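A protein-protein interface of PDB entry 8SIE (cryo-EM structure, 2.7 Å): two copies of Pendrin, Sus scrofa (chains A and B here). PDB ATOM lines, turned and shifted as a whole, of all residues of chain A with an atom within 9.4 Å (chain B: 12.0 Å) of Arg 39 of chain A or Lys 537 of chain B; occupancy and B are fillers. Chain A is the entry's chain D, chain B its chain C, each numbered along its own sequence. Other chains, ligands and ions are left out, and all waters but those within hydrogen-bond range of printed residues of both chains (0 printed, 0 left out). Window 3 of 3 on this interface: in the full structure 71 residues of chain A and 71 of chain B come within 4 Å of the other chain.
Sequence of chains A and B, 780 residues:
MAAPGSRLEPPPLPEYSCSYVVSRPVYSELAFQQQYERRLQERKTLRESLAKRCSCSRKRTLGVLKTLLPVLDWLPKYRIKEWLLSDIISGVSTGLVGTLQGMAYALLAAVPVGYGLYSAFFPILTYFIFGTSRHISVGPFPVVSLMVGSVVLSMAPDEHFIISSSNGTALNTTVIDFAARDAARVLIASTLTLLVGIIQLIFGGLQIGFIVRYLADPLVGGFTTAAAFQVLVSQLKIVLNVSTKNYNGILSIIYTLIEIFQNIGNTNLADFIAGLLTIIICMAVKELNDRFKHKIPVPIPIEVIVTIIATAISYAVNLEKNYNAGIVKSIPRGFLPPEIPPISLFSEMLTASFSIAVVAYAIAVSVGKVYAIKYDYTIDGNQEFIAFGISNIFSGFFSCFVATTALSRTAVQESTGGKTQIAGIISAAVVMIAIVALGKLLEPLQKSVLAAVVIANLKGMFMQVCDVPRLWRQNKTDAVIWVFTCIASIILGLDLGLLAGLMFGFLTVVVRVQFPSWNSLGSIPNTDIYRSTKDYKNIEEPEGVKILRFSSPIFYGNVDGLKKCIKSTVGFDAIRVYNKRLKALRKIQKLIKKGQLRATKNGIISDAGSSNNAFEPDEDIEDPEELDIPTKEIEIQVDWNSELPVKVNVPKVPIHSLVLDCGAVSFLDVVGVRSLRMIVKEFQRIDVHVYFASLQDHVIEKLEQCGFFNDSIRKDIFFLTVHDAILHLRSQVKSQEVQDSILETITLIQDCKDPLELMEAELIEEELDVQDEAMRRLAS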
ATOM      1  N   GLN A  33      -6.728  -9.054  26.723  1.00  0.00           N
ATOM      2  CA  GLN A  33      -5.670  -8.119  26.359  1.00  0.00           C
ATOM      3  C   GLN A  33      -4.336  -8.822  26.150  1.00  0.00           C
ATOM      4  O   GLN A  33      -3.536  -8.382  25.317  1.00  0.00           O
ATOM      5  CB  GLN A  33      -5.540  -7.027  27.419  1.00  0.00           C
ATOM      6  CG  GLN A  33      -6.713  -6.061  27.459  1.00  0.00           C
ATOM      7  CD  GLN A  33      -6.826  -5.229  26.199  1.00  0.00           C
ATOM      8  OE1 GLN A  33      -5.828  -4.731  25.680  1.00  0.00           O
ATOM      9  NE2 GLN A  33      -8.045  -5.074  25.699  1.00  0.00           N
ATOM     10  N   TYR A  36      -5.206 -10.878  22.564  1.00  0.00           N
ATOM     11  CA  TYR A  36      -5.339  -9.921  21.473  1.00  0.00           C
ATOM     12  C   TYR A  36      -4.835  -8.565  21.947  1.00  0.00           C
ATOM     13  O   TYR A  36      -5.365  -8.006  22.913  1.00  0.00           O
ATOM     14  CB  TYR A  36      -6.790  -9.817  21.003  1.00  0.00           C
ATOM     15  CG  TYR A  36      -7.400 -11.142  20.607  1.00  0.00           C
ATOM     16  CD1 TYR A  36      -7.179 -11.680  19.348  1.00  0.00           C
ATOM     17  CD2 TYR A  36      -8.194 -11.856  21.493  1.00  0.00           C
ATOM     18  CE1 TYR A  36      -7.731 -12.890  18.980  1.00  0.00           C
ATOM     19  CE2 TYR A  36      -8.752 -13.067  21.134  1.00  0.00           C
ATOM     20  CZ  TYR A  36      -8.517 -13.579  19.877  1.00  0.00           C
ATOM     21  OH  TYR A  36      -9.069 -14.785  19.515  1.00  0.00           O
ATOM     22  N   GLU A  37      -3.822  -8.041  21.266  1.00  0.00           N
ATOM     23  CA  GLU A  37      -3.154  -6.818  21.684  1.00  0.00           C
ATOM     24  C   GLU A  37      -3.804  -5.604  21.034  1.00  0.00           C
ATOM     25  O   GLU A  37      -4.198  -5.645  19.865  1.00  0.00           O
ATOM     26  CB  GLU A  37      -1.663  -6.869  21.343  1.00  0.00           C
ATOM     27  CG  GLU A  37      -1.352  -6.902  19.855  1.00  0.00           C
ATOM     28  CD  GLU A  37       0.132  -7.018  19.575  1.00  0.00           C
ATOM     29  OE1 GLU A  37       0.919  -7.094  20.541  1.00  0.00           O
ATOM     30  OE2 GLU A  37       0.514  -7.031  18.385  1.00  0.00           O
ATOM     31  N   ARG A  38      -3.920  -4.528  21.805  1.00  0.00           N
ATOM     32  CA  ARG A  38      -4.510  -3.288  21.322  1.00  0.00           C
ATOM     33  C   ARG A  38      -3.421  -2.470  20.622  1.00  0.00           C
ATOM     34  O   ARG A  38      -2.285  -2.925  20.455  1.00  0.00           O
ATOM     35  CB  ARG A  38      -5.168  -2.542  22.483  1.00  0.00           C
ATOM     36  CG  ARG A  38      -6.170  -1.476  22.070  1.00  0.00           C
ATOM     37  CD  ARG A  38      -6.786  -0.790  23.273  1.00  0.00           C
ATOM     38  NE  ARG A  38      -7.727   0.245  22.867  1.00  0.00           N
ATOM     39  CZ  ARG A  38      -8.345   1.066  23.703  1.00  0.00           C
ATOM     40  NH1 ARG A  38      -8.137   1.007  25.008  1.00  0.00           N
ATOM     41  NH2 ARG A  38      -9.187   1.975  23.219  1.00  0.00           N
ATOM     42  N   ARG A  39      -3.762  -1.254  20.195  1.00  0.00           N
ATOM     43  CA  ARG A  39      -2.838  -0.353  19.508  1.00  0.00           C
ATOM     44  C   ARG A  39      -2.258  -0.991  18.249  1.00  0.00           C
ATOM     45  O   ARG A  39      -2.486  -0.513  17.139  1.00  0.00           O
ATOM     46  CB  ARG A  39      -1.706   0.082  20.447  1.00  0.00           C
ATOM     47  CG  ARG A  39      -2.144   0.998  21.577  1.00  0.00           C
ATOM     48  CD  ARG A  39      -2.315   2.428  21.094  1.00  0.00           C
ATOM     49  NE  ARG A  39      -2.557   3.352  22.195  1.00  0.00           N
ATOM     50  CZ  ARG A  39      -2.966   4.604  22.047  1.00  0.00           C
ATOM     51  NH1 ARG A  39      -3.195   5.119  20.850  1.00  0.00           N
ATOM     52  NH2 ARG A  39      -3.152   5.358  23.126  1.00  0.00           N
ATOM     53  N   ASP A 697     -13.465   0.374  26.370  1.00  0.00           N
ATOM     54  CA  ASP A 697     -12.012   0.500  26.429  1.00  0.00           C
ATOM     55  C   ASP A 697     -11.584   1.858  26.972  1.00  0.00           C
ATOM     56  O   ASP A 697     -10.651   1.944  27.779  1.00  0.00           O
ATOM     57  CB  ASP A 697     -11.415   0.266  25.043  1.00  0.00           C
ATOM     58  CG  ASP A 697     -11.419  -1.193  24.648  1.00  0.00           C
ATOM     59  OD1 ASP A 697     -11.371  -2.053  25.552  1.00  0.00           O
ATOM     60  OD2 ASP A 697     -11.469  -1.481  23.434  1.00  0.00           O
ATOM     61  N   GLU A 701      -9.398   2.850  30.245  1.00  0.00           N
ATOM     62  CA  GLU A 701      -8.249   3.752  30.227  1.00  0.00           C
ATOM     63  C   GLU A 701      -8.391   4.846  31.276  1.00  0.00           C
ATOM     64  O   GLU A 701      -7.416   5.204  31.950  1.00  0.00           O
ATOM     65  CB  GLU A 701      -8.081   4.374  28.842  1.00  0.00           C
ATOM     66  CG  GLU A 701      -7.451   3.467  27.810  1.00  0.00           C
ATOM     67  CD  GLU A 701      -7.514   4.061  26.419  1.00  0.00           C
ATOM     68  OE1 GLU A 701      -7.431   3.295  25.439  1.00  0.00           O
ATOM     69  OE2 GLU A 701      -7.649   5.297  26.309  1.00  0.00           O
ATOM     70  N   GLU A 704      -7.560   3.429  34.514  1.00  0.00           N
ATOM     71  CA  GLU A 704      -6.116   3.251  34.634  1.00  0.00           C
ATOM     72  C   GLU A 704      -5.420   4.557  34.994  1.00  0.00           C
ATOM     73  O   GLU A 704      -4.551   4.583  35.873  1.00  0.00           O
ATOM     74  CB  GLU A 704      -5.542   2.699  33.329  1.00  0.00           C
ATOM     75  CG  GLU A 704      -5.586   1.190  33.204  1.00  0.00           C
ATOM     76  CD  GLU A 704      -5.445   0.730  31.768  1.00  0.00           C
ATOM     77  OE1 GLU A 704      -6.196  -0.175  31.354  1.00  0.00           O
ATOM     78  OE2 GLU A 704      -4.580   1.278  31.052  1.00  0.00           O
ATOM     79  N   GLN A 705      -5.785   5.653  34.328  1.00  0.00           N
ATOM     80  CA  GLN A 705      -5.101   6.919  34.551  1.00  0.00           C
ATOM     81  C   GLN A 705      -5.588   7.653  35.793  1.00  0.00           C
ATOM     82  O   GLN A 705      -4.994   8.673  36.159  1.00  0.00           O
ATOM     83  CB  GLN A 705      -5.244   7.824  33.324  1.00  0.00           C
ATOM     84  CG  GLN A 705      -6.598   8.488  33.183  1.00  0.00           C
ATOM     85  CD  GLN A 705      -6.680   9.362  31.949  1.00  0.00           C
ATOM     86  OE1 GLN A 705      -6.367  10.551  31.995  1.00  0.00           O
ATOM     87  NE2 GLN A 705      -7.098   8.775  30.835  1.00  0.00           N
ATOM     88  N   ASN B 519     -17.207   4.730  17.544  1.00  0.00           N
ATOM     89  CA  ASN B 519     -16.268   3.796  16.941  1.00  0.00           C
ATOM     90  C   ASN B 519     -16.920   3.048  15.788  1.00  0.00           C
ATOM     91  O   ASN B 519     -18.144   2.921  15.709  1.00  0.00           O
ATOM     92  CB  ASN B 519     -15.735   2.792  17.970  1.00  0.00           C
ATOM     93  CG  ASN B 519     -14.599   3.353  18.798  1.00  0.00           C
ATOM     94  OD1 ASN B 519     -13.684   3.983  18.270  1.00  0.00           O
ATOM     95  ND2 ASN B 519     -14.650   3.122  20.103  1.00  0.00           N
ATOM     96  N   SER B 520     -16.069   2.553  14.893  1.00  0.00           N
ATOM     97  CA  SER B 520     -16.457   1.615  13.849  1.00  0.00           C
ATOM     98  C   SER B 520     -15.976   0.227  14.251  1.00  0.00           C
ATOM     99  O   SER B 520     -14.792   0.038  14.547  1.00  0.00           O
ATOM    100  CB  SER B 520     -15.866   2.019  12.498  1.00  0.00           C
ATOM    101  OG  SER B 520     -16.222   1.094  11.488  1.00  0.00           O
ATOM    102  N   LEU B 521     -16.889  -0.737  14.254  1.00  0.00           N
ATOM    103  CA  LEU B 521     -16.668  -2.025  14.890  1.00  0.00           C
ATOM    104  C   LEU B 521     -16.505  -3.138  13.865  1.00  0.00           C
ATOM    105  O   LEU B 521     -17.115  -3.124  12.792  1.00  0.00           O
ATOM    106  CB  LEU B 521     -17.824  -2.373  15.833  1.00  0.00           C
ATOM    107  CG  LEU B 521     -18.116  -1.398  16.974  1.00  0.00           C
ATOM    108  CD1 LEU B 521     -19.035  -2.044  17.992  1.00  0.00           C
ATOM    109  CD2 LEU B 521     -16.831  -0.931  17.633  1.00  0.00           C
ATOM    110  N   GLY B 522     -15.657  -4.105  14.218  1.00  0.00           N
ATOM    111  CA  GLY B 522     -15.530  -5.332  13.466  1.00  0.00           C
ATOM    112  C   GLY B 522     -15.260  -6.482  14.414  1.00  0.00           C
ATOM    113  O   GLY B 522     -14.853  -6.283  15.562  1.00  0.00           O
ATOM    114  N   SER B 523     -15.478  -7.694  13.912  1.00  0.00           N
ATOM    115  CA  SER B 523     -15.518  -8.879  14.756  1.00  0.00           C
ATOM    116  C   SER B 523     -14.144  -9.511  14.922  1.00  0.00           C
ATOM    117  O   SER B 523     -13.355  -9.575  13.976  1.00  0.00           O
ATOM    118  CB  SER B 523     -16.483  -9.913  14.174  1.00  0.00           C
ATOM    119  OG  SER B 523     -16.498 -11.091  14.959  1.00  0.00           O
ATOM    120  N   ILE B 524     -13.866  -9.968  16.136  1.00  0.00           N
ATOM    121  CA  ILE B 524     -12.766 -10.914  16.356  1.00  0.00           C
ATOM    122  C   ILE B 524     -13.149 -12.255  15.740  1.00  0.00           C
ATOM    123  O   ILE B 524     -14.253 -12.760  16.011  1.00  0.00           O
ATOM    124  CB  ILE B 524     -12.476 -11.055  17.853  1.00  0.00           C
ATOM    125  CG1 ILE B 524     -11.872  -9.768  18.419  1.00  0.00           C
ATOM    126  CG2 ILE B 524     -11.547 -12.230  18.114  1.00  0.00           C
ATOM    127  CD1 ILE B 524     -10.439  -9.530  18.005  1.00  0.00           C
ATOM    128  N   PRO B 525     -12.301 -12.858  14.907  1.00  0.00           N
ATOM    129  CA  PRO B 525     -12.714 -14.067  14.181  1.00  0.00           C
ATOM    130  C   PRO B 525     -13.076 -15.214  15.115  1.00  0.00           C
ATOM    131  O   PRO B 525     -12.462 -15.404  16.167  1.00  0.00           O
ATOM    132  CB  PRO B 525     -11.487 -14.404  13.327  1.00  0.00           C
ATOM    133  CG  PRO B 525     -10.350 -13.677  13.964  1.00  0.00           C
ATOM    134  CD  PRO B 525     -10.936 -12.438  14.555  1.00  0.00           C
ATOM    135  N   ILE B 529     -17.323 -11.240  19.512  1.00  0.00           N
ATOM    136  CA  ILE B 529     -16.732 -10.058  20.125  1.00  0.00           C
ATOM    137  C   ILE B 529     -16.428  -9.047  19.032  1.00  0.00           C
ATOM    138  O   ILE B 529     -15.748  -9.369  18.050  1.00  0.00           O
ATOM    139  CB  ILE B 529     -15.460 -10.423  20.909  1.00  0.00           C
ATOM    140  CG1 ILE B 529     -15.788 -11.448  21.995  1.00  0.00           C
ATOM    141  CG2 ILE B 529     -14.824  -9.180  21.512  1.00  0.00           C
ATOM    142  CD1 ILE B 529     -14.582 -12.182  22.525  1.00  0.00           C
ATOM    143  N   TYR B 530     -16.931  -7.827  19.196  1.00  0.00           N
ATOM    144  CA  TYR B 530     -16.755  -6.761  18.218  1.00  0.00           C
ATOM    145  C   TYR B 530     -16.015  -5.604  18.872  1.00  0.00           C
ATOM    146  O   TYR B 530     -16.445  -5.095  19.912  1.00  0.00           O
ATOM    147  CB  TYR B 530     -18.103  -6.304  17.657  1.00  0.00           C
ATOM    148  CG  TYR B 530     -18.723  -7.298  16.702  1.00  0.00           C
ATOM    149  CD1 TYR B 530     -19.244  -8.499  17.161  1.00  0.00           C
ATOM    150  CD2 TYR B 530     -18.777  -7.042  15.341  1.00  0.00           C
ATOM    151  CE1 TYR B 530     -19.802  -9.414  16.293  1.00  0.00           C
ATOM    152  CE2 TYR B 530     -19.340  -7.950  14.466  1.00  0.00           C
ATOM    153  CZ  TYR B 530     -19.850  -9.134  14.950  1.00  0.00           C
ATOM    154  OH  TYR B 530     -20.408 -10.045  14.086  1.00  0.00           O
ATOM    155  N   ARG B 531     -14.907  -5.194  18.261  1.00  0.00           N
ATOM    156  CA  ARG B 531     -14.058  -4.132  18.776  1.00  0.00           C
ATOM    157  C   ARG B 531     -13.747  -3.147  17.659  1.00  0.00           C
ATOM    158  O   ARG B 531     -14.047  -3.389  16.488  1.00  0.00           O
ATOM    159  CB  ARG B 531     -12.753  -4.688  19.360  1.00  0.00           C
ATOM    160  CG  ARG B 531     -12.932  -5.589  20.566  1.00  0.00           C
ATOM    161  CD  ARG B 531     -13.421  -4.799  21.765  1.00  0.00           C
ATOM    162  NE  ARG B 531     -13.455  -5.613  22.973  1.00  0.00           N
ATOM    163  CZ  ARG B 531     -13.952  -5.209  24.132  1.00  0.00           C
ATOM    164  NH1 ARG B 531     -14.480  -4.004  24.276  1.00  0.00           N
ATOM    165  NH2 ARG B 531     -13.918  -6.033  25.174  1.00  0.00           N
ATOM    166  N   SER B 532     -13.129  -2.029  18.029  1.00  0.00           N
ATOM    167  CA  SER B 532     -12.765  -1.023  17.042  1.00  0.00           C
ATOM    168  C   SER B 532     -11.765  -1.592  16.042  1.00  0.00           C
ATOM    169  O   SER B 532     -10.824  -2.298  16.411  1.00  0.00           O
ATOM    170  CB  SER B 532     -12.181   0.208  17.733  1.00  0.00           C
ATOM    171  OG  SER B 532     -11.773   1.178  16.784  1.00  0.00           O
ATOM    172  N   THR B 533     -11.982  -1.281  14.763  1.00  0.00           N
ATOM    173  CA  THR B 533     -11.154  -1.856  13.706  1.00  0.00           C
ATOM    174  C   THR B 533      -9.733  -1.304  13.738  1.00  0.00           C
ATOM    175  O   THR B 533      -8.780  -2.016  13.403  1.00  0.00           O
ATOM    176  CB  THR B 533     -11.793  -1.600  12.342  1.00  0.00           C
ATOM    177  OG1 THR B 533     -13.202  -1.847  12.417  1.00  0.00           O
ATOM    178  CG2 THR B 533     -11.183  -2.511  11.291  1.00  0.00           C
ATOM    179  N   LYS B 534      -9.571  -0.047  14.135  1.00  0.00           N
ATOM    180  CA  LYS B 534      -8.280   0.622  14.085  1.00  0.00           C
ATOM    181  C   LYS B 534      -7.483   0.486  15.377  1.00  0.00           C
ATOM    182  O   LYS B 534      -6.482   1.189  15.545  1.00  0.00           O
ATOM    183  CB  LYS B 534      -8.470   2.103  13.746  1.00  0.00           C
ATOM    184  CG  LYS B 534      -9.226   2.888  14.802  1.00  0.00           C
ATOM    185  CD  LYS B 534      -9.403   4.338  14.387  1.00  0.00           C
ATOM    186  CE  LYS B 534     -10.208   5.114  15.417  1.00  0.00           C
ATOM    187  NZ  LYS B 534      -9.522   5.161  16.737  1.00  0.00           N
ATOM    188  N   ASP B 535      -7.895  -0.392  16.288  1.00  0.00           N
ATOM    189  CA  ASP B 535      -7.227  -0.534  17.577  1.00  0.00           C
ATOM    190  C   ASP B 535      -6.569  -1.887  17.797  1.00  0.00           C
ATOM    191  O   ASP B 535      -5.510  -1.948  18.421  1.00  0.00           O
ATOM    192  CB  ASP B 535      -8.217  -0.274  18.720  1.00  0.00           C
ATOM    193  CG  ASP B 535      -8.623   1.182  18.820  1.00  0.00           C
ATOM    194  OD1 ASP B 535      -7.818   2.052  18.426  1.00  0.00           O
ATOM    195  OD2 ASP B 535      -9.736   1.461  19.309  1.00  0.00           O
ATOM    196  N   TYR B 536      -7.155  -2.980  17.307  1.00  0.00           N
ATOM    197  CA  TYR B 536      -6.713  -4.308  17.703  1.00  0.00           C
ATOM    198  C   TYR B 536      -5.861  -5.029  16.666  1.00  0.00           C
ATOM    199  O   TYR B 536      -5.247  -6.048  17.002  1.00  0.00           O
ATOM    200  CB  TYR B 536      -7.926  -5.179  18.064  1.00  0.00           C
ATOM    201  CG  TYR B 536      -8.472  -4.866  19.437  1.00  0.00           C
ATOM    202  CD1 TYR B 536      -9.284  -3.760  19.645  1.00  0.00           C
ATOM    203  CD2 TYR B 536      -8.157  -5.661  20.528  1.00  0.00           C
ATOM    204  CE1 TYR B 536      -9.777  -3.464  20.899  1.00  0.00           C
ATOM    205  CE2 TYR B 536      -8.644  -5.372  21.785  1.00  0.00           C
ATOM    206  CZ  TYR B 536      -9.455  -4.272  21.964  1.00  0.00           C
ATOM    207  OH  TYR B 536      -9.945  -3.980  23.215  1.00  0.00           O
ATOM    208  N   LYS B 537      -5.814  -4.547  15.425  1.00  0.00           N
ATOM    209  CA  LYS B 537      -4.950  -5.039  14.353  1.00  0.00           C
ATOM    210  C   LYS B 537      -5.282  -6.460  13.910  1.00  0.00           C
ATOM    211  O   LYS B 537      -4.637  -6.969  12.987  1.00  0.00           O
ATOM    212  CB  LYS B 537      -3.460  -4.978  14.727  1.00  0.00           C
ATOM    213  CG  LYS B 537      -2.987  -3.609  15.195  1.00  0.00           C
ATOM    214  CD  LYS B 537      -3.101  -2.573  14.089  1.00  0.00           C
ATOM    215  CE  LYS B 537      -4.122  -1.500  14.436  1.00  0.00           C
ATOM    216  NZ  LYS B 537      -4.204  -0.453  13.382  1.00  0.00           N
ATOM    217  N   ASN B 538      -6.262  -7.117  14.530  1.00  0.00           N
ATOM    218  CA  ASN B 538      -6.737  -8.425  14.095  1.00  0.00           C
ATOM    219  C   ASN B 538      -8.240  -8.414  13.855  1.00  0.00           C
ATOM    220  O   ASN B 538      -8.889  -9.463  13.919  1.00  0.00           O
ATOM    221  CB  ASN B 538      -6.365  -9.501  15.117  1.00  0.00           C
ATOM    222  CG  ASN B 538      -6.120 -10.855  14.476  1.00  0.00           C
ATOM    223  OD1 ASN B 538      -6.414 -11.059  13.298  1.00  0.00           O
ATOM    224  ND2 ASN B 538      -5.579 -11.787  15.251  1.00  0.00           N
ATOM    225  N   ILE B 539      -8.800  -7.241  13.580  1.00  0.00           N
ATOM    226  CA  ILE B 539     -10.235  -7.050  13.419  1.00  0.00           C
ATOM    227  C   ILE B 539     -10.571  -7.104  11.937  1.00  0.00           C
ATOM    228  O   ILE B 539      -9.937  -6.420  11.124  1.00  0.00           O
ATOM    229  CB  ILE B 539     -10.682  -5.714  14.036  1.00  0.00           C
ATOM    230  CG1 ILE B 539     -10.604  -5.769  15.562  1.00  0.00           C
ATOM    231  CG2 ILE B 539     -12.074  -5.361  13.581  1.00  0.00           C
ATOM    232  CD1 ILE B 539     -11.627  -6.676  16.188  1.00  0.00           C
ATOM    233  N   GLU B 540     -11.566  -7.911  11.584  1.00  0.00           N
ATOM    234  CA  GLU B 540     -12.019  -8.044  10.206  1.00  0.00           C
ATOM    235  C   GLU B 540     -13.368  -7.353  10.055  1.00  0.00           C
ATOM    236  O   GLU B 540     -14.322  -7.678  10.772  1.00  0.00           O
ATOM    237  CB  GLU B 540     -12.116  -9.515   9.799  1.00  0.00           C
ATOM    238  CG  GLU B 540     -12.810 -10.407  10.817  1.00  0.00           C
ATOM    239  CD  GLU B 540     -12.707 -11.875  10.465  1.00  0.00           C
ATOM    240  OE1 GLU B 540     -11.617 -12.311  10.036  1.00  0.00           O
ATOM    241  OE2 GLU B 540     -13.717 -12.594  10.614  1.00  0.00           O
ATOM    242  N   GLU B 541     -13.441  -6.395   9.138  1.00  0.00           N
ATOM    243  CA  GLU B 541     -14.717  -5.774   8.825  1.00  0.00           C
ATOM    244  C   GLU B 541     -15.580  -6.749   8.028  1.00  0.00           C
ATOM    245  O   GLU B 541     -15.089  -7.399   7.101  1.00  0.00           O
ATOM    246  CB  GLU B 541     -14.511  -4.486   8.032  1.00  0.00           C
ATOM    247  CG  GLU B 541     -13.392  -3.606   8.557  1.00  0.00           C
ATOM    248  CD  GLU B 541     -13.559  -2.152   8.158  1.00  0.00           C
ATOM    249  OE1 GLU B 541     -14.683  -1.626   8.288  1.00  0.00           O
ATOM    250  OE2 GLU B 541     -12.565  -1.537   7.717  1.00  0.00           O
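Of the 20 printed residues of chain B, 5 touch a printed residue of chain A. Hydrophobic or aromatic side chains of chain B that line the printed part of chain A: Ile 524 and Tyr 536. Along chain B the printed residues that touch a printed residue of chain A span positions 524 to 537. Of the 9 printed residues of chain A, 6 touch a printed residue of chain B. Along chain A the printed residues that touch a printed residue of chain B span positions 33 to 697. Among the printed residues, 8 pairs touch across the chains. Among the printed residues, Asp or Glu carboxylates within 4 Å of a Lys or Arg side-chain nitrogen of the other chain: Arg 38 of chain A with Asp 535 of chain B (3.98 Å) and Asp 697 of chain A with Arg 531 of chain B (3.9 Å).
Of the printed residues of chain B, Tyr 36 of chain A touches Ile 524. Of the printed residues of chain B, Glu 37 of chain A touches Tyr 536. Arg 38 of chain A touches just one residue of chain B: Asp 535. Arg 39 of chain A touches just these residues of chain B: Asp 535 (2.6 Å) and Lys 537 (3.3 Å). Of the printed residues of chain B, Asp 697 of chain A touches Arg 531 and Tyr 536. Ser 520 of chain B touches none of the printed residues of chain A. Gly 522 of chain B touches none of the printed residues of chain A. Of the printed residues of chain A, Asp 535 of chain B touches Arg 38 (3.1 Å) and Arg 39 (2.6 Å). Lys 537 of chain B touches just one residue of chain A: Arg 39 (3.3 Å). The nearest residue of chain B that does not touch Arg 39 of chain A is Lys 534 of chain B (4.6 Å).
NE2 of Gln 33 of chain A sits at hydrogen-bond distance from OH of Tyr 536 of chain B (3.3 Å). The guanidinium group of Arg 38 of chain A lies within salt-bridge range of the side-chain carboxylate of Asp 535 of chain B, 3.98 Å away. The backbone carbonyl oxygen of Asp 535 of chain B is in hydrogen-bond range of the backbone NH of Arg 39 of chain A. The guanidinium group (NH1) of Arg 531 of chain B lies within salt-bridge range of the side-chain carboxylate (OD1) of Asp 697 of chain A, at 3.9 Å. The side-chain hydroxyl (OH) of Tyr 536 of chain B is in hydrogen-bond range of the side-chain carboxylate (OD2) of Asp 697 of chain A (2.9 Å). O of Tyr 536 of chain B sits close to O of Glu 37 of chain A (3.1 Å).
The side-chain carboxylate of Glu 701 of chain A lies within salt-bridge range of the guanidinium group of Arg 38 of chain A (2.4 Å). The backbone NH (N) of Gly 522 of chain B is in hydrogen-bond range of the backbone carbonyl oxygen (O) of Arg 531 of chain B (2.9 Å). N of Ile 524 of chain B lies within hydrogen-bond range of O of Ile 529 of chain B (2.8 Å). OD2 of Asp 535 of chain B sits close to OG of Ser 532 of chain B, at 3.3 Å. NZ of Lys 534 of chain B lies within salt-bridge range of OD1 of Asp 535 of chain B.
No position is printed for both chains. Of the 8 pairs that touch across the chains among the printed residues, none has its exchanged pair printed and touching as well.
CZ of Tyr 36 of chain A touches CG2 of Ile 524 of chain B, at 3.8 Å. Arg 39 of chain A touches Lys 537 of chain B (O to CE, 3.3 Å).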
